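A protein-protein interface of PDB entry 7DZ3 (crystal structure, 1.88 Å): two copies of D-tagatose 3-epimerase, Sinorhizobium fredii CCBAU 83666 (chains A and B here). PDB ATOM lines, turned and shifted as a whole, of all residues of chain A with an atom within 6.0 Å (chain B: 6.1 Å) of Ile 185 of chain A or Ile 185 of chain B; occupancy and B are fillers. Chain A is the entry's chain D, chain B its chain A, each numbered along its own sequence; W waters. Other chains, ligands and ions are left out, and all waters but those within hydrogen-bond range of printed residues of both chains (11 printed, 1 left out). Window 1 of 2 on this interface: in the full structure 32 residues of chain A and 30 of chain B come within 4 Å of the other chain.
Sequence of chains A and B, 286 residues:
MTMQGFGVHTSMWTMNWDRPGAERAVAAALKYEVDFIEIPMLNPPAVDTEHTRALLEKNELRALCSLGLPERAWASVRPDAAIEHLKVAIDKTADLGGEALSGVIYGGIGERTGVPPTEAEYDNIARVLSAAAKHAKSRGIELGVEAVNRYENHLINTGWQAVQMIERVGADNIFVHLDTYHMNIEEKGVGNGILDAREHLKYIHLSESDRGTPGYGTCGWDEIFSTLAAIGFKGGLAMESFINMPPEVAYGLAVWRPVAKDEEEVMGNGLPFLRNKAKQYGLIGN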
ATOM      1  N   ASN A 149     -20.160 -16.019   9.988  1.00  0.00           N
ATOM      2  CA  ASN A 149     -19.958 -17.052   8.980  1.00  0.00           C
ATOM      3  C   ASN A 149     -20.640 -18.383   9.365  1.00  0.00           C
ATOM      4  O   ASN A 149     -21.050 -18.620  10.514  1.00  0.00           O
ATOM      5  CB  ASN A 149     -18.454 -17.262   8.727  1.00  0.00           C
ATOM      6  CG  ASN A 149     -17.754 -17.985   9.867  1.00  0.00           C
ATOM      7  OD1 ASN A 149     -17.963 -19.174  10.081  1.00  0.00           O
ATOM      8  ND2 ASN A 149     -16.873 -17.282  10.560  1.00  0.00           N
ATOM      9  N   ARG A 150     -20.734 -19.246   8.347  1.00  0.00           N
ATOM     10  CA  ARG A 150     -21.474 -20.499   8.374  1.00  0.00           C
ATOM     11  C   ARG A 150     -21.067 -21.402   9.513  1.00  0.00           C
ATOM     12  O   ARG A 150     -21.869 -22.240   9.958  1.00  0.00           O
ATOM     13  CB  ARG A 150     -21.241 -21.232   7.052  1.00  0.00           C
ATOM     14  CG  ARG A 150     -19.765 -21.552   6.832  1.00  0.00           C
ATOM     15  CD  ARG A 150     -19.397 -21.841   5.354  1.00  0.00           C
ATOM     16  NE  ARG A 150     -19.818 -20.715   4.520  1.00  0.00           N
ATOM     17  CZ  ARG A 150     -20.024 -20.787   3.209  1.00  0.00           C
ATOM     18  NH1 ARG A 150     -19.829 -21.924   2.571  1.00  0.00           N
ATOM     19  NH2 ARG A 150     -20.405 -19.713   2.539  1.00  0.00           N
ATOM     20  N   TYR A 151     -19.841 -21.251   9.994  1.00  0.00           N
ATOM     21  CA  TYR A 151     -19.346 -22.121  11.051  1.00  0.00           C
ATOM     22  C   TYR A 151     -19.704 -21.639  12.439  1.00  0.00           C
ATOM     23  O   TYR A 151     -19.589 -22.417  13.395  1.00  0.00           O
ATOM     24  CB  TYR A 151     -17.828 -22.232  10.991  1.00  0.00           C
ATOM     25  CG  TYR A 151     -17.270 -22.853   9.759  1.00  0.00           C
ATOM     26  CD1 TYR A 151     -17.410 -24.204   9.508  1.00  0.00           C
ATOM     27  CD2 TYR A 151     -16.558 -22.079   8.842  1.00  0.00           C
ATOM     28  CE1 TYR A 151     -16.858 -24.789   8.384  1.00  0.00           C
ATOM     29  CE2 TYR A 151     -16.013 -22.634   7.719  1.00  0.00           C
ATOM     30  CZ  TYR A 151     -16.160 -23.977   7.479  1.00  0.00           C
ATOM     31  OH  TYR A 151     -15.593 -24.507   6.359  1.00  0.00           O
ATOM     32  N   THR A 180     -15.814  -7.855   8.476  1.00  0.00           N
ATOM     33  CA  THR A 180     -15.042  -8.189   7.282  1.00  0.00           C
ATOM     34  C   THR A 180     -14.458  -9.594   7.369  1.00  0.00           C
ATOM     35  O   THR A 180     -14.318 -10.276   6.334  1.00  0.00           O
ATOM     36  CB  THR A 180     -13.927  -7.168   7.067  1.00  0.00           C
ATOM     37  OG1 THR A 180     -13.158  -7.012   8.272  1.00  0.00           O
ATOM     38  CG2 THR A 180     -14.504  -5.793   6.687  1.00  0.00           C
ATOM     39  N   TYR A 181     -14.132 -10.046   8.583  1.00  0.00           N
ATOM     40  CA  TYR A 181     -13.694 -11.430   8.779  1.00  0.00           C
ATOM     41  C   TYR A 181     -14.757 -12.403   8.311  1.00  0.00           C
ATOM     42  O   TYR A 181     -14.472 -13.387   7.615  1.00  0.00           O
ATOM     43  CB  TYR A 181     -13.372 -11.658  10.261  1.00  0.00           C
ATOM     44  CG  TYR A 181     -13.237 -13.108  10.675  1.00  0.00           C
ATOM     45  CD1 TYR A 181     -12.009 -13.750  10.612  1.00  0.00           C
ATOM     46  CD2 TYR A 181     -14.326 -13.810  11.197  1.00  0.00           C
ATOM     47  CE1 TYR A 181     -11.866 -15.089  11.041  1.00  0.00           C
ATOM     48  CE2 TYR A 181     -14.196 -15.129  11.609  1.00  0.00           C
ATOM     49  CZ  TYR A 181     -12.955 -15.754  11.536  1.00  0.00           C
ATOM     50  OH  TYR A 181     -12.816 -17.048  11.964  1.00  0.00           O
ATOM     51  N   HIS A 182     -15.996 -12.169   8.723  1.00  0.00           N
ATOM     52  CA  HIS A 182     -17.081 -13.030   8.291  1.00  0.00           C
ATOM     53  C   HIS A 182     -17.399 -12.841   6.809  1.00  0.00           C
ATOM     54  O   HIS A 182     -17.634 -13.811   6.092  1.00  0.00           O
ATOM     55  CB  HIS A 182     -18.307 -12.751   9.138  1.00  0.00           C
ATOM     56  CG  HIS A 182     -18.126 -13.136  10.562  1.00  0.00           C
ATOM     57  ND1 HIS A 182     -17.773 -14.422  10.945  1.00  0.00           N
ATOM     58  CD2 HIS A 182     -18.242 -12.413  11.701  1.00  0.00           C
ATOM     59  CE1 HIS A 182     -17.676 -14.466  12.263  1.00  0.00           C
ATOM     60  NE2 HIS A 182     -17.964 -13.267  12.746  1.00  0.00           N
ATOM     61  N   MET A 183     -17.385 -11.601   6.321  1.00  0.00           N
ATOM     62  CA  MET A 183     -17.679 -11.377   4.906  1.00  0.00           C
ATOM     63  C   MET A 183     -16.623 -11.988   3.999  1.00  0.00           C
ATOM     64  O   MET A 183     -16.931 -12.425   2.892  1.00  0.00           O
ATOM     65  CB  MET A 183     -17.798  -9.876   4.670  1.00  0.00           C
ATOM     66  CG  MET A 183     -19.074  -9.286   5.247  1.00  0.00           C
ATOM     67  SD  MET A 183     -19.352  -7.587   4.623  1.00  0.00           S
ATOM     68  CE  MET A 183     -18.015  -6.786   5.441  1.00  0.00           C
ATOM     69  N   ASN A 184     -15.386 -12.057   4.474  1.00  0.00           N
ATOM     70  CA  ASN A 184     -14.309 -12.680   3.730  1.00  0.00           C
ATOM     71  C   ASN A 184     -14.652 -14.107   3.333  1.00  0.00           C
ATOM     72  O   ASN A 184     -14.171 -14.587   2.308  1.00  0.00           O
ATOM     73  CB  ASN A 184     -13.049 -12.615   4.600  1.00  0.00           C
ATOM     74  CG  ASN A 184     -11.835 -13.151   3.900  1.00  0.00           C
ATOM     75  OD1 ASN A 184     -11.483 -12.728   2.792  1.00  0.00           O
ATOM     76  ND2 ASN A 184     -11.164 -14.084   4.562  1.00  0.00           N
ATOM     77  N   ILE A 185     -15.481 -14.783   4.123  1.00  0.00           N
ATOM     78  CA  ILE A 185     -15.935 -16.144   3.844  1.00  0.00           C
ATOM     79  C   ILE A 185     -17.276 -16.147   3.125  1.00  0.00           C
ATOM     80  O   ILE A 185     -17.457 -16.885   2.164  1.00  0.00           O
ATOM     81  CB  ILE A 185     -16.058 -16.925   5.173  1.00  0.00           C
ATOM     82  CG1 ILE A 185     -14.727 -17.061   5.883  1.00  0.00           C
ATOM     83  CG2 ILE A 185     -16.570 -18.339   4.948  1.00  0.00           C
ATOM     84  CD1 ILE A 185     -14.843 -17.453   7.369  1.00  0.00           C
ATOM     85  N   GLU A 186     -18.221 -15.317   3.575  1.00  0.00           N
ATOM     86  CA  GLU A 186     -19.614 -15.460   3.170  1.00  0.00           C
ATOM     87  C   GLU A 186     -20.018 -14.645   1.951  1.00  0.00           C
ATOM     88  O   GLU A 186     -20.930 -15.068   1.225  1.00  0.00           O
ATOM     89  CB  GLU A 186     -20.541 -15.062   4.306  1.00  0.00           C
ATOM     90  CG  GLU A 186     -20.322 -15.940   5.538  1.00  0.00           C
ATOM     91  CD  GLU A 186     -20.615 -17.427   5.271  1.00  0.00           C
ATOM     92  OE1 GLU A 186     -21.465 -17.741   4.417  1.00  0.00           O
ATOM     93  OE2 GLU A 186     -19.956 -18.284   5.897  1.00  0.00           O
ATOM     94  N   GLU A 187     -19.421 -13.482   1.722  1.00  0.00           N
ATOM     95  CA  GLU A 187     -19.894 -12.614   0.656  1.00  0.00           C
ATOM     96  C   GLU A 187     -19.206 -12.957  -0.659  1.00  0.00           C
ATOM     97  O   GLU A 187     -17.994 -13.186  -0.718  1.00  0.00           O
ATOM     98  CB  GLU A 187     -19.683 -11.145   1.000  1.00  0.00           C
ATOM     99  CG  GLU A 187     -20.343 -10.645   2.298  1.00  0.00           C
ATOM    100  CD  GLU A 187     -21.855 -10.693   2.328  1.00  0.00           C
ATOM    101  OE1 GLU A 187     -22.475 -10.851   1.248  1.00  0.00           O
ATOM    102  OE2 GLU A 187     -22.430 -10.550   3.448  1.00  0.00           O
ATOM    103  N   SER A 209      -8.690 -11.249   8.202  1.00  0.00           N
ATOM    104  CA  SER A 209      -9.220 -12.552   7.791  1.00  0.00           C
ATOM    105  C   SER A 209      -8.879 -13.663   8.781  1.00  0.00           C
ATOM    106  O   SER A 209      -9.614 -14.649   8.883  1.00  0.00           O
ATOM    107  CB  SER A 209      -8.659 -12.925   6.413  1.00  0.00           C
ATOM    108  OG  SER A 209      -7.256 -12.693   6.442  1.00  0.00           O
ATOM    109  N   ASP A 210      -7.771 -13.531   9.491  1.00  0.00           N
ATOM    110  CA  ASP A 210      -7.395 -14.485  10.528  1.00  0.00           C
ATOM    111  C   ASP A 210      -7.554 -13.924  11.946  1.00  0.00           C
ATOM    112  O   ASP A 210      -6.988 -14.473  12.884  1.00  0.00           O
ATOM    113  CB  ASP A 210      -5.962 -14.945  10.258  1.00  0.00           C
ATOM    114  CG  ASP A 210      -4.938 -13.827  10.478  1.00  0.00           C
ATOM    115  OD1 ASP A 210      -5.288 -12.616  10.560  1.00  0.00           O
ATOM    116  OD2 ASP A 210      -3.750 -14.181  10.591  1.00  0.00           O
ATOM    117  N   ARG A 211      -8.371 -12.891  12.125  1.00  0.00           N
ATOM    118  CA  ARG A 211      -8.598 -12.156  13.369  1.00  0.00           C
ATOM    119  C   ARG A 211      -7.357 -11.459  13.889  1.00  0.00           C
ATOM    120  O   ARG A 211      -7.375 -10.940  15.005  1.00  0.00           O
ATOM    121  CB  ARG A 211      -9.187 -13.052  14.493  1.00  0.00           C
ATOM    122  CG  ARG A 211     -10.550 -13.648  14.148  1.00  0.00           C
ATOM    123  CD  ARG A 211     -11.616 -12.574  14.055  1.00  0.00           C
ATOM    124  NE  ARG A 211     -12.956 -13.103  14.344  1.00  0.00           N
ATOM    125  CZ  ARG A 211     -14.086 -12.414  14.222  1.00  0.00           C
ATOM    126  NH1 ARG A 211     -14.071 -11.128  13.806  1.00  0.00           N
ATOM    127  NH2 ARG A 211     -15.246 -13.004  14.521  1.00  0.00           N
ATOM    128  N   THR A 218      -6.047 -11.403   4.389  1.00  0.00           N
ATOM    129  CA  THR A 218      -6.534 -11.523   3.025  1.00  0.00           C
ATOM    130  C   THR A 218      -7.742 -10.654   2.731  1.00  0.00           C
ATOM    131  O   THR A 218      -8.283 -10.744   1.627  1.00  0.00           O
ATOM    132  CB  THR A 218      -6.893 -12.975   2.691  1.00  0.00           C
ATOM    133  OG1 THR A 218      -8.090 -13.352   3.394  1.00  0.00           O
ATOM    134  CG2 THR A 218      -5.766 -13.916   3.065  1.00  0.00           C
ATOM    135  N   ARG A 257      -4.712 -20.618  18.353  1.00  0.00           N
ATOM    136  CA  ARG A 257      -3.335 -20.163  18.314  1.00  0.00           C
ATOM    137  C   ARG A 257      -3.381 -18.647  18.274  1.00  0.00           C
ATOM    138  O   ARG A 257      -4.421 -18.067  17.921  1.00  0.00           O
ATOM    139  CB  ARG A 257      -2.590 -20.719  17.093  1.00  0.00           C
ATOM    140  CG  ARG A 257      -3.226 -20.286  15.778  1.00  0.00           C
ATOM    141  CD  ARG A 257      -2.797 -21.110  14.585  1.00  0.00           C
ATOM    142  NE  ARG A 257      -3.537 -20.709  13.378  1.00  0.00           N
ATOM    143  CZ  ARG A 257      -3.180 -19.733  12.562  1.00  0.00           C
ATOM    144  NH1 ARG A 257      -2.059 -19.030  12.792  1.00  0.00           N
ATOM    145  NH2 ARG A 257      -3.948 -19.470  11.517  1.00  0.00           N
ATOM    146  N   ASN B 149      -9.463 -25.248   7.849  1.00  0.00           N
ATOM    147  CA  ASN B 149      -9.584 -24.101   8.726  1.00  0.00           C
ATOM    148  C   ASN B 149      -9.991 -24.502  10.143  1.00  0.00           C
ATOM    149  O   ASN B 149     -10.510 -25.602  10.412  1.00  0.00           O
ATOM    150  CB  ASN B 149     -10.579 -23.091   8.163  1.00  0.00           C
ATOM    151  CG  ASN B 149     -12.018 -23.555   8.241  1.00  0.00           C
ATOM    152  OD1 ASN B 149     -12.627 -23.647   9.326  1.00  0.00           O
ATOM    153  ND2 ASN B 149     -12.584 -23.842   7.070  1.00  0.00           N
ATOM    154  N   ARG B 150      -9.840 -23.518  11.027  1.00  0.00           N
ATOM    155  CA  ARG B 150     -10.011 -23.686  12.462  1.00  0.00           C
ATOM    156  C   ARG B 150     -11.335 -24.299  12.858  1.00  0.00           C
ATOM    157  O   ARG B 150     -11.435 -24.936  13.920  1.00  0.00           O
ATOM    158  CB  ARG B 150      -9.897 -22.301  13.120  1.00  0.00           C
ATOM    159  CG  ARG B 150     -10.923 -21.291  12.480  1.00  0.00           C
ATOM    160  CD  ARG B 150     -10.549 -19.838  12.799  1.00  0.00           C
ATOM    161  NE  ARG B 150      -9.224 -19.550  12.270  1.00  0.00           N
ATOM    162  CZ  ARG B 150      -8.476 -18.504  12.609  1.00  0.00           C
ATOM    163  NH1 ARG B 150      -8.934 -17.607  13.452  1.00  0.00           N
ATOM    164  NH2 ARG B 150      -7.276 -18.366  12.079  1.00  0.00           N
ATOM    165  N   TYR B 151     -12.385 -24.074  12.067  1.00  0.00           N
ATOM    166  CA  TYR B 151     -13.699 -24.557  12.470  1.00  0.00           C
ATOM    167  C   TYR B 151     -13.904 -26.043  12.148  1.00  0.00           C
ATOM    168  O   TYR B 151     -14.774 -26.702  12.755  1.00  0.00           O
ATOM    169  CB  TYR B 151     -14.791 -23.741  11.796  1.00  0.00           C
ATOM    170  CG  TYR B 151     -14.798 -22.256  12.101  1.00  0.00           C
ATOM    171  CD1 TYR B 151     -15.303 -21.772  13.304  1.00  0.00           C
ATOM    172  CD2 TYR B 151     -14.355 -21.331  11.161  1.00  0.00           C
ATOM    173  CE1 TYR B 151     -15.353 -20.416  13.572  1.00  0.00           C
ATOM    174  CE2 TYR B 151     -14.402 -19.959  11.415  1.00  0.00           C
ATOM    175  CZ  TYR B 151     -14.908 -19.505  12.619  1.00  0.00           C
ATOM    176  OH  TYR B 151     -14.977 -18.147  12.860  1.00  0.00           O
ATOM    177  N   THR B 180      -7.188 -23.095  -1.159  1.00  0.00           N
ATOM    178  CA  THR B 180      -7.304 -21.641  -1.106  1.00  0.00           C
ATOM    179  C   THR B 180      -8.488 -21.181  -0.270  1.00  0.00           C
ATOM    180  O   THR B 180      -8.425 -20.105   0.339  1.00  0.00           O
ATOM    181  CB  THR B 180      -7.401 -21.091  -2.530  1.00  0.00           C
ATOM    182  OG1 THR B 180      -8.468 -21.723  -3.239  1.00  0.00           O
ATOM    183  CG2 THR B 180      -6.139 -21.393  -3.273  1.00  0.00           C
ATOM    184  N   TYR B 181      -9.560 -21.978  -0.195  1.00  0.00           N
ATOM    185  CA  TYR B 181     -10.665 -21.626   0.692  1.00  0.00           C
ATOM    186  C   TYR B 181     -10.226 -21.608   2.145  1.00  0.00           C
ATOM    187  O   TYR B 181     -10.606 -20.717   2.907  1.00  0.00           O
ATOM    188  CB  TYR B 181     -11.806 -22.619   0.479  1.00  0.00           C
ATOM    189  CG  TYR B 181     -12.890 -22.644   1.517  1.00  0.00           C
ATOM    190  CD1 TYR B 181     -13.994 -21.795   1.429  1.00  0.00           C
ATOM    191  CD2 TYR B 181     -12.856 -23.558   2.560  1.00  0.00           C
ATOM    192  CE1 TYR B 181     -15.016 -21.851   2.349  1.00  0.00           C
ATOM    193  CE2 TYR B 181     -13.862 -23.632   3.468  1.00  0.00           C
ATOM    194  CZ  TYR B 181     -14.935 -22.781   3.387  1.00  0.00           C
ATOM    195  OH  TYR B 181     -15.941 -22.900   4.328  1.00  0.00           O
ATOM    196  N   HIS B 182      -9.428 -22.592   2.553  1.00  0.00           N
ATOM    197  CA  HIS B 182      -8.956 -22.642   3.932  1.00  0.00           C
ATOM    198  C   HIS B 182      -7.898 -21.586   4.173  1.00  0.00           C
ATOM    199  O   HIS B 182      -7.914 -20.905   5.211  1.00  0.00           O
ATOM    200  CB  HIS B 182      -8.430 -24.055   4.233  1.00  0.00           C
ATOM    201  CG  HIS B 182      -9.505 -25.105   4.223  1.00  0.00           C
ATOM    202  ND1 HIS B 182     -10.655 -24.988   4.976  1.00  0.00           N
ATOM    203  CD2 HIS B 182      -9.610 -26.281   3.555  1.00  0.00           C
ATOM    204  CE1 HIS B 182     -11.427 -26.046   4.779  1.00  0.00           C
ATOM    205  NE2 HIS B 182     -10.814 -26.850   3.923  1.00  0.00           N
ATOM    206  N   MET B 183      -6.989 -21.427   3.209  1.00  0.00           N
ATOM    207  CA  MET B 183      -5.938 -20.437   3.315  1.00  0.00           C
ATOM    208  C   MET B 183      -6.482 -19.019   3.375  1.00  0.00           C
ATOM    209  O   MET B 183      -5.890 -18.156   4.028  1.00  0.00           O
ATOM    210  CB  MET B 183      -5.009 -20.545   2.121  1.00  0.00           C
ATOM    211  CG  MET B 183      -4.277 -21.879   1.912  1.00  0.00           C
ATOM    212  SD  MET B 183      -3.600 -21.885   0.211  1.00  0.00           S
ATOM    213  CE  MET B 183      -2.135 -21.130   0.765  1.00  0.00           C
ATOM    214  N   ASN B 184      -7.595 -18.767   2.686  1.00  0.00           N
ATOM    215  CA  ASN B 184      -8.261 -17.466   2.701  1.00  0.00           C
ATOM    216  C   ASN B 184      -8.620 -17.037   4.110  1.00  0.00           C
ATOM    217  O   ASN B 184      -8.680 -15.832   4.390  1.00  0.00           O
ATOM    218  CB  ASN B 184      -9.511 -17.564   1.816  1.00  0.00           C
ATOM    219  CG  ASN B 184     -10.240 -16.244   1.683  1.00  0.00           C
ATOM    220  OD1 ASN B 184     -11.448 -16.136   1.937  1.00  0.00           O
ATOM    221  ND2 ASN B 184      -9.521 -15.252   1.284  1.00  0.00           N
ATOM    222  N   ILE B 185      -8.856 -18.009   4.994  1.00  0.00           N
ATOM    223  CA  ILE B 185      -9.111 -17.773   6.413  1.00  0.00           C
ATOM    224  C   ILE B 185      -7.823 -17.843   7.216  1.00  0.00           C
ATOM    225  O   ILE B 185      -7.555 -17.005   8.072  1.00  0.00           O
ATOM    226  CB  ILE B 185     -10.129 -18.802   6.947  1.00  0.00           C
ATOM    227  CG1 ILE B 185     -11.422 -18.825   6.130  1.00  0.00           C
ATOM    228  CG2 ILE B 185     -10.458 -18.550   8.429  1.00  0.00           C
ATOM    229  CD1 ILE B 185     -12.300 -20.062   6.434  1.00  0.00           C
ATOM    230  N   GLU B 186      -6.994 -18.855   6.957  1.00  0.00           N
ATOM    231  CA  GLU B 186      -5.927 -19.170   7.914  1.00  0.00           C
ATOM    232  C   GLU B 186      -4.599 -18.466   7.679  1.00  0.00           C
ATOM    233  O   GLU B 186      -3.847 -18.270   8.638  1.00  0.00           O
ATOM    234  CB  GLU B 186      -5.688 -20.687   7.936  1.00  0.00           C
ATOM    235  CG  GLU B 186      -6.928 -21.490   8.415  1.00  0.00           C
ATOM    236  CD  GLU B 186      -7.342 -21.148   9.847  1.00  0.00           C
ATOM    237  OE1 GLU B 186      -6.452 -20.798  10.660  1.00  0.00           O
ATOM    238  OE2 GLU B 186      -8.547 -21.198  10.157  1.00  0.00           O
ATOM    239  N   GLU B 187      -4.261 -18.111   6.446  1.00  0.00           N
ATOM    240  CA  GLU B 187      -2.905 -17.667   6.145  1.00  0.00           C
ATOM    241  C   GLU B 187      -2.802 -16.148   6.271  1.00  0.00           C
ATOM    242  O   GLU B 187      -3.722 -15.410   5.890  1.00  0.00           O
ATOM    243  CB  GLU B 187      -2.477 -18.124   4.761  1.00  0.00           C
ATOM    244  CG  GLU B 187      -2.536 -19.643   4.589  1.00  0.00           C
ATOM    245  CD  GLU B 187      -1.541 -20.447   5.436  1.00  0.00           C
ATOM    246  OE1 GLU B 187      -0.615 -19.855   6.021  1.00  0.00           O
ATOM    247  OE2 GLU B 187      -1.676 -21.693   5.492  1.00  0.00           O
ATOM    248  N   SER B 209     -13.605 -18.541  -2.097  1.00  0.00           N
ATOM    249  CA  SER B 209     -13.761 -18.264  -0.688  1.00  0.00           C
ATOM    250  C   SER B 209     -15.086 -18.727  -0.114  1.00  0.00           C
ATOM    251  O   SER B 209     -15.177 -18.904   1.102  1.00  0.00           O
ATOM    252  CB  SER B 209     -13.620 -16.754  -0.449  1.00  0.00           C
ATOM    253  OG  SER B 209     -14.519 -16.041  -1.307  1.00  0.00           O
ATOM    254  N   ASP B 210     -16.119 -18.860  -0.936  1.00  0.00           N
ATOM    255  CA  ASP B 210     -17.426 -19.339  -0.481  1.00  0.00           C
ATOM    256  C   ASP B 210     -17.761 -20.720  -1.021  1.00  0.00           C
ATOM    257  O   ASP B 210     -18.924 -21.120  -1.011  1.00  0.00           O
ATOM    258  CB  ASP B 210     -18.523 -18.325  -0.885  1.00  0.00           C
ATOM    259  CG  ASP B 210     -18.660 -18.174  -2.397  1.00  0.00           C
ATOM    260  OD1 ASP B 210     -17.779 -18.650  -3.149  1.00  0.00           O
ATOM    261  OD2 ASP B 210     -19.670 -17.576  -2.850  1.00  0.00           O
ATOM    262  N   ARG B 211     -16.780 -21.434  -1.544  1.00  0.00           N
ATOM    263  CA  ARG B 211     -16.924 -22.727  -2.206  1.00  0.00           C
ATOM    264  C   ARG B 211     -17.723 -22.619  -3.498  1.00  0.00           C
ATOM    265  O   ARG B 211     -18.142 -23.625  -4.039  1.00  0.00           O
ATOM    266  CB  ARG B 211     -17.548 -23.760  -1.271  1.00  0.00           C
ATOM    267  CG  ARG B 211     -16.672 -24.082  -0.052  1.00  0.00           C
ATOM    268  CD  ARG B 211     -15.323 -24.668  -0.463  1.00  0.00           C
ATOM    269  NE  ARG B 211     -14.699 -25.470   0.603  1.00  0.00           N
ATOM    270  CZ  ARG B 211     -13.506 -26.070   0.484  1.00  0.00           C
ATOM    271  NH1 ARG B 211     -12.826 -25.955  -0.647  1.00  0.00           N
ATOM    272  NH2 ARG B 211     -13.026 -26.803   1.489  1.00  0.00           N
ATOM    273  N   THR B 218     -13.557 -13.827  -2.749  1.00  0.00           N
ATOM    274  CA  THR B 218     -12.528 -13.004  -2.137  1.00  0.00           C
ATOM    275  C   THR B 218     -11.134 -13.591  -2.212  1.00  0.00           C
ATOM    276  O   THR B 218     -10.206 -12.971  -1.689  1.00  0.00           O
ATOM    277  CB  THR B 218     -12.859 -12.728  -0.671  1.00  0.00           C
ATOM    278  OG1 THR B 218     -12.730 -13.928   0.100  1.00  0.00           O
ATOM    279  CG2 THR B 218     -14.260 -12.187  -0.557  1.00  0.00           C
ATOM    280  N   ARG B 257     -26.815 -23.016   2.298  1.00  0.00           N
ATOM    281  CA  ARG B 257     -27.445 -22.295   1.201  1.00  0.00           C
ATOM    282  C   ARG B 257     -26.642 -22.572  -0.055  1.00  0.00           C
ATOM    283  O   ARG B 257     -25.479 -22.981   0.032  1.00  0.00           O
ATOM    284  CB  ARG B 257     -27.519 -20.786   1.482  1.00  0.00           C
ATOM    285  CG  ARG B 257     -26.156 -20.079   1.680  1.00  0.00           C
ATOM    286  CD  ARG B 257     -26.288 -18.708   2.341  1.00  0.00           C
ATOM    287  NE  ARG B 257     -24.942 -18.184   2.602  1.00  0.00           N
ATOM    288  CZ  ARG B 257     -24.233 -17.445   1.755  1.00  0.00           C
ATOM    289  NH1 ARG B 257     -24.729 -17.096   0.577  1.00  0.00           N
ATOM    290  NH2 ARG B 257     -23.018 -17.044   2.103  1.00  0.00           N
HETATM  291  O   HOH W   1      -2.611 -16.822  10.523  1.00  0.00           O
HETATM  292  O   HOH W   2     -23.446 -19.453   4.575  1.00  0.00           O
HETATM  293  O   HOH W   3     -16.831 -15.532  -0.161  1.00  0.00           O
HETATM  294  O   HOH W   4      -6.109 -15.010   6.993  1.00  0.00           O
HETATM  295  O   HOH W   5     -22.992 -15.167  -0.831  1.00  0.00           O
HETATM  296  O   HOH W   6      -5.250 -16.587  13.425  1.00  0.00           O
HETATM  297  O   HOH W   7     -21.406 -20.085  -0.126  1.00  0.00           O
HETATM  298  O   HOH W   8     -11.377 -17.146  14.585  1.00  0.00           O
HETATM  299  O   HOH W   9     -14.134 -15.609  15.063  1.00  0.00           O
HETATM  300  O   HOH W  10     -18.317 -24.538   3.301  1.00  0.00           O
HETATM  301  O   HOH W  11      -6.143 -21.741  13.149  1.00  0.00           O
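ND2 of Asn 149 of chain B lies within hydrogen-bond range of OH of Tyr 151 of chain A (3.2 Å).
The side-chain hydroxyl (OH) of Tyr 151 of chain B lies within hydrogen-bond range of the side-chain hydroxyl (OH) of Tyr 181 of chain A, 2.6 Å away.
The side-chain hydroxyl (OH) of Tyr 181 of chain B is in hydrogen-bond range of the side-chain hydroxyl (OH) of Tyr 151 of chain A.
The backbone carbonyl oxygen (O) of Asn 184 of chain B sits at hydrogen-bond distance from the side-chain amide nitrogen (ND2) of Asn 184 of chain A (3.0 Å).
The backbone carbonyl oxygen (O) of Asn 184 of chain B sits at hydrogen-bond distance from the side-chain hydroxyl (OG1) of Thr 218 of chain A (2.7 Å).
The guanidinium group (NH2) of Arg 257 of chain A is in salt-bridge range of the side-chain carboxylate (OE1) of Glu 186 of chain B, 3.0 Å away.
The side-chain hydroxyl (OG1) of Thr 218 of chain B sits at hydrogen-bond distance from the backbone carbonyl oxygen (O) of Asn 184 of chain A, at 2.7 Å.
The guanidinium group (NH2) of Arg 257 of chain B is in salt-bridge range of the side-chain carboxylate (OE1) of Glu 186 of chain A.
O of Ile 185 of chain A sits close to O of Ser 209 of chain B (3.2 Å).
O of Ser 209 of chain A sits close to O of Ile 185 of chain B (3.2 Å).
A ring nitrogen (ND1) of His 182 of chain B is in hydrogen-bond range of the side-chain amide nitrogen (ND2) of Asn 149 of chain B (3.1 Å).
Arg 150 of chain A touches Asp 210 of chain B (NH1 to O, 3.8 Å).
Tyr 151 of chain A touches Tyr 151 of chain B.
Glu 187 of chain A touches Thr 218 of chain B.
O of Ile 185 of chain B touches CB of Asp 210 of chain A, 3.4 Å away.
Printed residues of chain A within 4 Å of Arg 150 of chain B: Tyr 181, Asp 210 and Arg 257.
Thr 180 of chain B touches none of the printed residues of chain A.
Of the printed residues of chain A, Arg 257 of chain B touches Arg 150 and Glu 186.
The nearest printed residue of chain A that does not touch Glu 186 of chain B is Asp 210 of chain A (4.3 Å).
Of the 16 printed residues of chain B, 12 touch a printed residue of chain A.
Hydrophobic or aromatic side chains of chain B within 4 Å of the printed part of chain A: Tyr 151, Tyr 181 and Ile 185.
Of the 16 printed residues of chain A, 12 touch a printed residue of chain B.
Hydrophobic or aromatic side chains of chain A that line the printed part of chain B: Tyr 151, Tyr 181 and Ile 185.
Among the printed residues, Asp or Glu carboxylates within 4 Å of a Lys or Arg side-chain nitrogen of the other chain: Glu 186 of chain A with Arg 257 of chain B and Arg 257 of chain A with Glu 186 of chain B.
Asn 184 of chain B touches its own counterpart, Asn 184 of chain A.
Of the 25 pairs that touch across the chains among the printed residues, 25 have their exchanged pair printed and touching as well.
Water W9 bridges the guanidinium group (NE) of Arg 211 of chain A and the side-chain hydroxyl (OH) of Tyr 151 of chain B.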
